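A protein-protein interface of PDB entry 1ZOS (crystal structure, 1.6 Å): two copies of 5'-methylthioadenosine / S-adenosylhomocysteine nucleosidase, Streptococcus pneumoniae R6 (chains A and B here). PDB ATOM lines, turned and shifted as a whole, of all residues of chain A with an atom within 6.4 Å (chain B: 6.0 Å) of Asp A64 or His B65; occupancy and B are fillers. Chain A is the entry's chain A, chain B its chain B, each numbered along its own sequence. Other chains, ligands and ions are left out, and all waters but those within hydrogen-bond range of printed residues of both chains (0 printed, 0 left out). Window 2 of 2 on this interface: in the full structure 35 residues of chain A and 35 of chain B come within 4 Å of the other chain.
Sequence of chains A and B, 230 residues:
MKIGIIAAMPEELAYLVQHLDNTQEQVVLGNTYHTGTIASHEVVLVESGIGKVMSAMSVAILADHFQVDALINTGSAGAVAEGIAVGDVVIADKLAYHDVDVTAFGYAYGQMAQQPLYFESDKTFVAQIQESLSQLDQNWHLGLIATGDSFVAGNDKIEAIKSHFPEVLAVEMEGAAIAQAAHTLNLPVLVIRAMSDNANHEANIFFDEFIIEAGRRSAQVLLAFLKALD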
ATOM      1  N   VAL A  59     -34.332 -22.206 -17.712  1.00  0.00           N
ATOM      2  CA  VAL A  59     -33.546 -22.925 -16.715  1.00  0.00           C
ATOM      3  C   VAL A  59     -32.091 -23.013 -17.159  1.00  0.00           C
ATOM      4  O   VAL A  59     -31.175 -22.747 -16.378  1.00  0.00           O
ATOM      5  CB  VAL A  59     -34.078 -24.357 -16.483  1.00  0.00           C
ATOM      6  CG1 VAL A  59     -33.087 -25.151 -15.629  1.00  0.00           C
ATOM      7  CG2 VAL A  59     -35.430 -24.301 -15.794  1.00  0.00           C
ATOM      8  N   ALA A  60     -31.888 -23.387 -18.418  1.00  0.00           N
ATOM      9  CA  ALA A  60     -30.547 -23.522 -18.970  1.00  0.00           C
ATOM     10  C   ALA A  60     -29.754 -22.223 -18.873  1.00  0.00           C
ATOM     11  O   ALA A  60     -28.582 -22.230 -18.498  1.00  0.00           O
ATOM     12  CB  ALA A  60     -30.627 -23.974 -20.426  1.00  0.00           C
ATOM     13  N   ILE A  61     -30.397 -21.113 -19.211  1.00  0.00           N
ATOM     14  CA  ILE A  61     -29.737 -19.815 -19.170  1.00  0.00           C
ATOM     15  C   ILE A  61     -29.474 -19.372 -17.732  1.00  0.00           C
ATOM     16  O   ILE A  61     -28.426 -18.793 -17.438  1.00  0.00           O
ATOM     17  CB  ILE A  61     -30.568 -18.766 -19.939  1.00  0.00           C
ATOM     18  CG1 ILE A  61     -30.616 -19.167 -21.420  1.00  0.00           C
ATOM     19  CG2 ILE A  61     -29.956 -17.375 -19.787  1.00  0.00           C
ATOM     20  CD1 ILE A  61     -31.612 -18.404 -22.253  1.00  0.00           C
ATOM     21  N   LEU A  62     -30.406 -19.659 -16.828  1.00  0.00           N
ATOM     22  CA  LEU A  62     -30.213 -19.289 -15.429  1.00  0.00           C
ATOM     23  C   LEU A  62     -28.985 -20.005 -14.881  1.00  0.00           C
ATOM     24  O   LEU A  62     -28.201 -19.433 -14.120  1.00  0.00           O
ATOM     25  CB  LEU A  62     -31.453 -19.651 -14.604  1.00  0.00           C
ATOM     26  CG  LEU A  62     -32.645 -18.708 -14.790  1.00  0.00           C
ATOM     27  CD1 LEU A  62     -33.883 -19.297 -14.132  1.00  0.00           C
ATOM     28  CD2 LEU A  62     -32.317 -17.346 -14.190  1.00  0.00           C
ATOM     29  N   ALA A  63     -28.812 -21.259 -15.283  1.00  0.00           N
ATOM     30  CA  ALA A  63     -27.674 -22.047 -14.828  1.00  0.00           C
ATOM     31  C   ALA A  63     -26.373 -21.629 -15.514  1.00  0.00           C
ATOM     32  O   ALA A  63     -25.376 -21.341 -14.851  1.00  0.00           O
ATOM     33  CB  ALA A  63     -27.941 -23.532 -15.077  1.00  0.00           C
ATOM     34  N   ASP A  64     -26.393 -21.582 -16.842  1.00  0.00           N
ATOM     35  CA  ASP A  64     -25.206 -21.236 -17.622  1.00  0.00           C
ATOM     36  C   ASP A  64     -24.740 -19.781 -17.514  1.00  0.00           C
ATOM     37  O   ASP A  64     -23.543 -19.513 -17.410  1.00  0.00           O
ATOM     38  CB  ASP A  64     -25.444 -21.569 -19.100  1.00  0.00           C
ATOM     39  CG  ASP A  64     -24.173 -21.486 -19.932  1.00  0.00           C
ATOM     40  OD1 ASP A  64     -23.228 -22.250 -19.647  1.00  0.00           O
ATOM     41  OD2 ASP A  64     -24.120 -20.666 -20.874  1.00  0.00           O
ATOM     42  N   HIS A  65     -25.682 -18.847 -17.538  1.00  0.00           N
ATOM     43  CA  HIS A  65     -25.341 -17.431 -17.495  1.00  0.00           C
ATOM     44  C   HIS A  65     -25.297 -16.811 -16.104  1.00  0.00           C
ATOM     45  O   HIS A  65     -24.491 -15.913 -15.851  1.00  0.00           O
ATOM     46  CB  HIS A  65     -26.323 -16.648 -18.373  1.00  0.00           C
ATOM     47  CG  HIS A  65     -25.796 -15.330 -18.849  1.00  0.00           C
ATOM     48  ND1 HIS A  65     -25.637 -14.242 -18.018  1.00  0.00           N
ATOM     49  CD2 HIS A  65     -25.391 -14.928 -20.077  1.00  0.00           C
ATOM     50  CE1 HIS A  65     -25.159 -13.226 -18.715  1.00  0.00           C
ATOM     51  NE2 HIS A  65     -25.001 -13.616 -19.966  1.00  0.00           N
ATOM     52  N   PHE A  66     -26.148 -17.285 -15.199  1.00  0.00           N
ATOM     53  CA  PHE A  66     -26.181 -16.719 -13.855  1.00  0.00           C
ATOM     54  C   PHE A  66     -25.729 -17.649 -12.739  1.00  0.00           C
ATOM     55  O   PHE A  66     -25.698 -17.252 -11.574  1.00  0.00           O
ATOM     56  CB  PHE A  66     -27.584 -16.191 -13.551  1.00  0.00           C
ATOM     57  CG  PHE A  66     -28.023 -15.096 -14.477  1.00  0.00           C
ATOM     58  CD1 PHE A  66     -28.640 -15.392 -15.688  1.00  0.00           C
ATOM     59  CD2 PHE A  66     -27.781 -13.763 -14.157  1.00  0.00           C
ATOM     60  CE1 PHE A  66     -29.010 -14.376 -16.570  1.00  0.00           C
ATOM     61  CE2 PHE A  66     -28.145 -12.737 -15.031  1.00  0.00           C
ATOM     62  CZ  PHE A  66     -28.762 -13.044 -16.241  1.00  0.00           C
ATOM     63  N   GLN A  67     -25.374 -18.878 -13.096  1.00  0.00           N
ATOM     64  CA  GLN A  67     -24.909 -19.865 -12.129  1.00  0.00           C
ATOM     65  C   GLN A  67     -25.809 -20.010 -10.901  1.00  0.00           C
ATOM     66  O   GLN A  67     -25.326 -20.014  -9.769  1.00  0.00           O
ATOM     67  CB  GLN A  67     -23.482 -19.528 -11.674  1.00  0.00           C
ATOM     68  CG  GLN A  67     -22.441 -19.605 -12.785  1.00  0.00           C
ATOM     69  CD  GLN A  67     -22.438 -18.380 -13.680  1.00  0.00           C
ATOM     70  OE1 GLN A  67     -22.060 -18.454 -14.851  1.00  0.00           O
ATOM     71  NE2 GLN A  67     -22.841 -17.241 -13.129  1.00  0.00           N
ATOM     72  N   VAL A  68     -27.116 -20.136 -11.119  1.00  0.00           N
ATOM     73  CA  VAL A  68     -28.037 -20.291  -9.995  1.00  0.00           C
ATOM     74  C   VAL A  68     -27.795 -21.628  -9.296  1.00  0.00           C
ATOM     75  O   VAL A  68     -27.297 -22.574  -9.906  1.00  0.00           O
ATOM     76  CB  VAL A  68     -29.508 -20.215 -10.450  1.00  0.00           C
ATOM     77  CG1 VAL A  68     -29.799 -18.837 -11.016  1.00  0.00           C
ATOM     78  CG2 VAL A  68     -29.797 -21.299 -11.486  1.00  0.00           C
ATOM     79  N   LEU A 185     -29.551 -30.825 -14.135  1.00  0.00           N
ATOM     80  CA  LEU A 185     -28.460 -29.988 -13.655  1.00  0.00           C
ATOM     81  C   LEU A 185     -28.126 -30.266 -12.193  1.00  0.00           C
ATOM     82  O   LEU A 185     -27.271 -29.599 -11.608  1.00  0.00           O
ATOM     83  CB  LEU A 185     -28.834 -28.517 -13.829  1.00  0.00           C
ATOM     84  CG  LEU A 185     -29.102 -28.095 -15.278  1.00  0.00           C
ATOM     85  CD1 LEU A 185     -29.731 -26.714 -15.303  1.00  0.00           C
ATOM     86  CD2 LEU A 185     -27.795 -28.117 -16.067  1.00  0.00           C
ATOM     87  N   GLN B  26     -15.366 -30.486 -24.549  1.00  0.00           N
ATOM     88  CA  GLN B  26     -15.461 -29.598 -23.398  1.00  0.00           C
ATOM     89  C   GLN B  26     -16.693 -30.005 -22.608  1.00  0.00           C
ATOM     90  O   GLN B  26     -17.710 -30.364 -23.194  1.00  0.00           O
ATOM     91  CB  GLN B  26     -15.649 -28.147 -23.841  1.00  0.00           C
ATOM     92  CG  GLN B  26     -14.547 -27.574 -24.700  1.00  0.00           C
ATOM     93  CD  GLN B  26     -14.858 -26.155 -25.132  1.00  0.00           C
ATOM     94  OE1 GLN B  26     -15.191 -25.304 -24.305  1.00  0.00           O
ATOM     95  NE2 GLN B  26     -14.748 -25.892 -26.428  1.00  0.00           N
ATOM     96  N   VAL B  28     -19.683 -28.820 -20.324  1.00  0.00           N
ATOM     97  CA  VAL B  28     -20.440 -27.655 -19.892  1.00  0.00           C
ATOM     98  C   VAL B  28     -21.740 -28.141 -19.268  1.00  0.00           C
ATOM     99  O   VAL B  28     -22.518 -28.855 -19.903  1.00  0.00           O
ATOM    100  CB  VAL B  28     -20.764 -26.716 -21.074  1.00  0.00           C
ATOM    101  CG1 VAL B  28     -21.591 -25.532 -20.591  1.00  0.00           C
ATOM    102  CG2 VAL B  28     -19.471 -26.233 -21.720  1.00  0.00           C
ATOM    103  N   LEU B  29     -21.965 -27.753 -18.018  1.00  0.00           N
ATOM    104  CA  LEU B  29     -23.158 -28.156 -17.290  1.00  0.00           C
ATOM    105  C   LEU B  29     -23.389 -29.659 -17.359  1.00  0.00           C
ATOM    106  O   LEU B  29     -24.507 -30.121 -17.585  1.00  0.00           O
ATOM    107  CB  LEU B  29     -24.383 -27.401 -17.812  1.00  0.00           C
ATOM    108  CG  LEU B  29     -24.393 -25.904 -17.488  1.00  0.00           C
ATOM    109  CD1 LEU B  29     -25.661 -25.264 -18.037  1.00  0.00           C
ATOM    110  CD2 LEU B  29     -24.308 -25.702 -15.977  1.00  0.00           C
ATOM    111  N   ALA B  60     -30.348 -23.540 -25.998  1.00  0.00           N
ATOM    112  CA  ALA B  60     -30.056 -22.395 -25.141  1.00  0.00           C
ATOM    113  C   ALA B  60     -28.575 -22.285 -24.791  1.00  0.00           C
ATOM    114  O   ALA B  60     -28.000 -21.197 -24.827  1.00  0.00           O
ATOM    115  CB  ALA B  60     -30.888 -22.479 -23.859  1.00  0.00           C
ATOM    116  N   ILE B  61     -27.963 -23.413 -24.451  1.00  0.00           N
ATOM    117  CA  ILE B  61     -26.555 -23.433 -24.079  1.00  0.00           C
ATOM    118  C   ILE B  61     -25.659 -23.177 -25.287  1.00  0.00           C
ATOM    119  O   ILE B  61     -24.641 -22.490 -25.178  1.00  0.00           O
ATOM    120  CB  ILE B  61     -26.191 -24.776 -23.408  1.00  0.00           C
ATOM    121  CG1 ILE B  61     -26.983 -24.913 -22.101  1.00  0.00           C
ATOM    122  CG2 ILE B  61     -24.692 -24.846 -23.137  1.00  0.00           C
ATOM    123  CD1 ILE B  61     -26.874 -26.263 -21.428  1.00  0.00           C
ATOM    124  N   LEU B  62     -26.035 -23.720 -26.442  1.00  0.00           N
ATOM    125  CA  LEU B  62     -25.243 -23.504 -27.647  1.00  0.00           C
ATOM    126  C   LEU B  62     -25.192 -22.013 -27.960  1.00  0.00           C
ATOM    127  O   LEU B  62     -24.141 -21.475 -28.310  1.00  0.00           O
ATOM    128  CB  LEU B  62     -25.847 -24.276 -28.826  1.00  0.00           C
ATOM    129  CG  LEU B  62     -25.546 -25.778 -28.809  1.00  0.00           C
ATOM    130  CD1 LEU B  62     -26.362 -26.488 -29.877  1.00  0.00           C
ATOM    131  CD2 LEU B  62     -24.048 -25.995 -29.036  1.00  0.00           C
ATOM    132  N   ALA B  63     -26.327 -21.343 -27.809  1.00  0.00           N
ATOM    133  CA  ALA B  63     -26.404 -19.914 -28.078  1.00  0.00           C
ATOM    134  C   ALA B  63     -25.731 -19.071 -26.990  1.00  0.00           C
ATOM    135  O   ALA B  63     -24.938 -18.175 -27.290  1.00  0.00           O
ATOM    136  CB  ALA B  63     -27.864 -19.495 -28.232  1.00  0.00           C
ATOM    137  N   ASP B  64     -26.035 -19.366 -25.729  1.00  0.00           N
ATOM    138  CA  ASP B  64     -25.479 -18.603 -24.610  1.00  0.00           C
ATOM    139  C   ASP B  64     -24.000 -18.846 -24.315  1.00  0.00           C
ATOM    140  O   ASP B  64     -23.264 -17.909 -23.998  1.00  0.00           O
ATOM    141  CB  ASP B  64     -26.280 -18.885 -23.333  1.00  0.00           C
ATOM    142  CG  ASP B  64     -25.889 -17.969 -22.183  1.00  0.00           C
ATOM    143  OD1 ASP B  64     -26.078 -16.746 -22.315  1.00  0.00           O
ATOM    144  OD2 ASP B  64     -25.395 -18.469 -21.151  1.00  0.00           O
ATOM    145  N   HIS B  65     -23.566 -20.094 -24.417  1.00  0.00           N
ATOM    146  CA  HIS B  65     -22.183 -20.440 -24.108  1.00  0.00           C
ATOM    147  C   HIS B  65     -21.236 -20.449 -25.306  1.00  0.00           C
ATOM    148  O   HIS B  65     -20.062 -20.104 -25.168  1.00  0.00           O
ATOM    149  CB  HIS B  65     -22.148 -21.802 -23.407  1.00  0.00           C
ATOM    150  CG  HIS B  65     -20.902 -22.050 -22.614  1.00  0.00           C
ATOM    151  ND1 HIS B  65     -19.676 -22.292 -23.199  1.00  0.00           N
ATOM    152  CD2 HIS B  65     -20.694 -22.097 -21.277  1.00  0.00           C
ATOM    153  CE1 HIS B  65     -18.771 -22.482 -22.256  1.00  0.00           C
ATOM    154  NE2 HIS B  65     -19.362 -22.369 -21.080  1.00  0.00           N
ATOM    155  N   PHE B  66     -21.737 -20.831 -26.476  1.00  0.00           N
ATOM    156  CA  PHE B  66     -20.888 -20.889 -27.662  1.00  0.00           C
ATOM    157  C   PHE B  66     -21.212 -19.864 -28.743  1.00  0.00           C
ATOM    158  O   PHE B  66     -20.517 -19.785 -29.754  1.00  0.00           O
ATOM    159  CB  PHE B  66     -20.923 -22.299 -28.261  1.00  0.00           C
ATOM    160  CG  PHE B  66     -20.411 -23.363 -27.330  1.00  0.00           C
ATOM    161  CD1 PHE B  66     -21.265 -23.991 -26.426  1.00  0.00           C
ATOM    162  CD2 PHE B  66     -19.063 -23.716 -27.334  1.00  0.00           C
ATOM    163  CE1 PHE B  66     -20.785 -24.957 -25.537  1.00  0.00           C
ATOM    164  CE2 PHE B  66     -18.571 -24.679 -26.450  1.00  0.00           C
ATOM    165  CZ  PHE B  66     -19.433 -25.302 -25.547  1.00  0.00           C
ATOM    166  N   GLN B  67     -22.259 -19.077 -28.527  1.00  0.00           N
ATOM    167  CA  GLN B  67     -22.664 -18.053 -29.483  1.00  0.00           C
ATOM    168  C   GLN B  67     -22.804 -18.564 -30.918  1.00  0.00           C
ATOM    169  O   GLN B  67     -22.276 -17.961 -31.853  1.00  0.00           O
ATOM    170  CB  GLN B  67     -21.676 -16.879 -29.462  1.00  0.00           C
ATOM    171  CG  GLN B  67     -21.637 -16.124 -28.140  1.00  0.00           C
ATOM    172  CD  GLN B  67     -20.831 -16.842 -27.078  1.00  0.00           C
ATOM    173  OE1 GLN B  67     -21.148 -16.770 -25.891  1.00  0.00           O
ATOM    174  NE2 GLN B  67     -19.771 -17.523 -27.498  1.00  0.00           N
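The backbone carbonyl oxygen (O) of Asp A64 lies close to the side-chain amide oxygen (OE1) of Gln A67, 3.1 Å away.
O of His A65 lies within hydrogen-bond range of NE2 of Gln A67 (3.4 Å).
The side-chain amide oxygen (OE1) of Gln B67 lies close to the backbone carbonyl oxygen (O) of Asp B64, at 3.1 Å.
O of His B65 sits at hydrogen-bond distance from NE2 of Gln B67 (3.5 Å).
The side-chain carboxylate of Asp B64 sits close to the side-chain carboxylate of Asp A64, at 2.6 Å.
Printed residues of chain A that touch a printed residue of chain B: Ala A60, Asp A64, His A65 and Leu A185.
Hydrophobic or aromatic side chains of chain B that line the printed part of chain A: Val B28, Leu B29, Ala B60 and His B65.
Among the printed residues, 7 pairs touch across the chains.
Among the printed residues, no Asp or Glu carboxylate lies within 4 Å of a Lys or Arg side-chain nitrogen of the other chain.
Asp A64 touches just these residues of chain B: Val B28, Leu B29, Asp B64 and His B65.
His B65 touches one residue of chain A.
Of the printed residues of chain A, Asp B64 touches Asp A64 (2.6 Å) and His A65 (3.0 Å).
Of the printed residues of chain B, Leu A185 touches Leu B29 (3.9 Å).
Printed residues of chain A within 4 Å of Leu B29: Asp A64 (3.9 Å) and Leu A185 (3.9 Å).
Of the printed residues of chain A, Ala B60 touches Ala A60 (3.8 Å).
Ala A60 touches its own counterpart, Ala B60.
Asp A64 touches its own counterpart, Asp B64.
Asp A64 touches His B65, and with the chains exchanged His A65 touches Asp B64.
8 positions are printed for both chains.
Ala B60 touches Ala A60 (CB to CB, 3.8 Å).
Asp A64 touches Val B28 (OD1 to CG1, 3.8 Å).
Asp A64 touches Leu B29.
Asp A64 touches His B65 (OD1 to CD2, 3.0 Å).
Asp B64 touches His A65 (OD1 to CD2, 3.0 Å).
Leu A185 touches Leu B29 (CD2 to CB, 3.9 Å).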
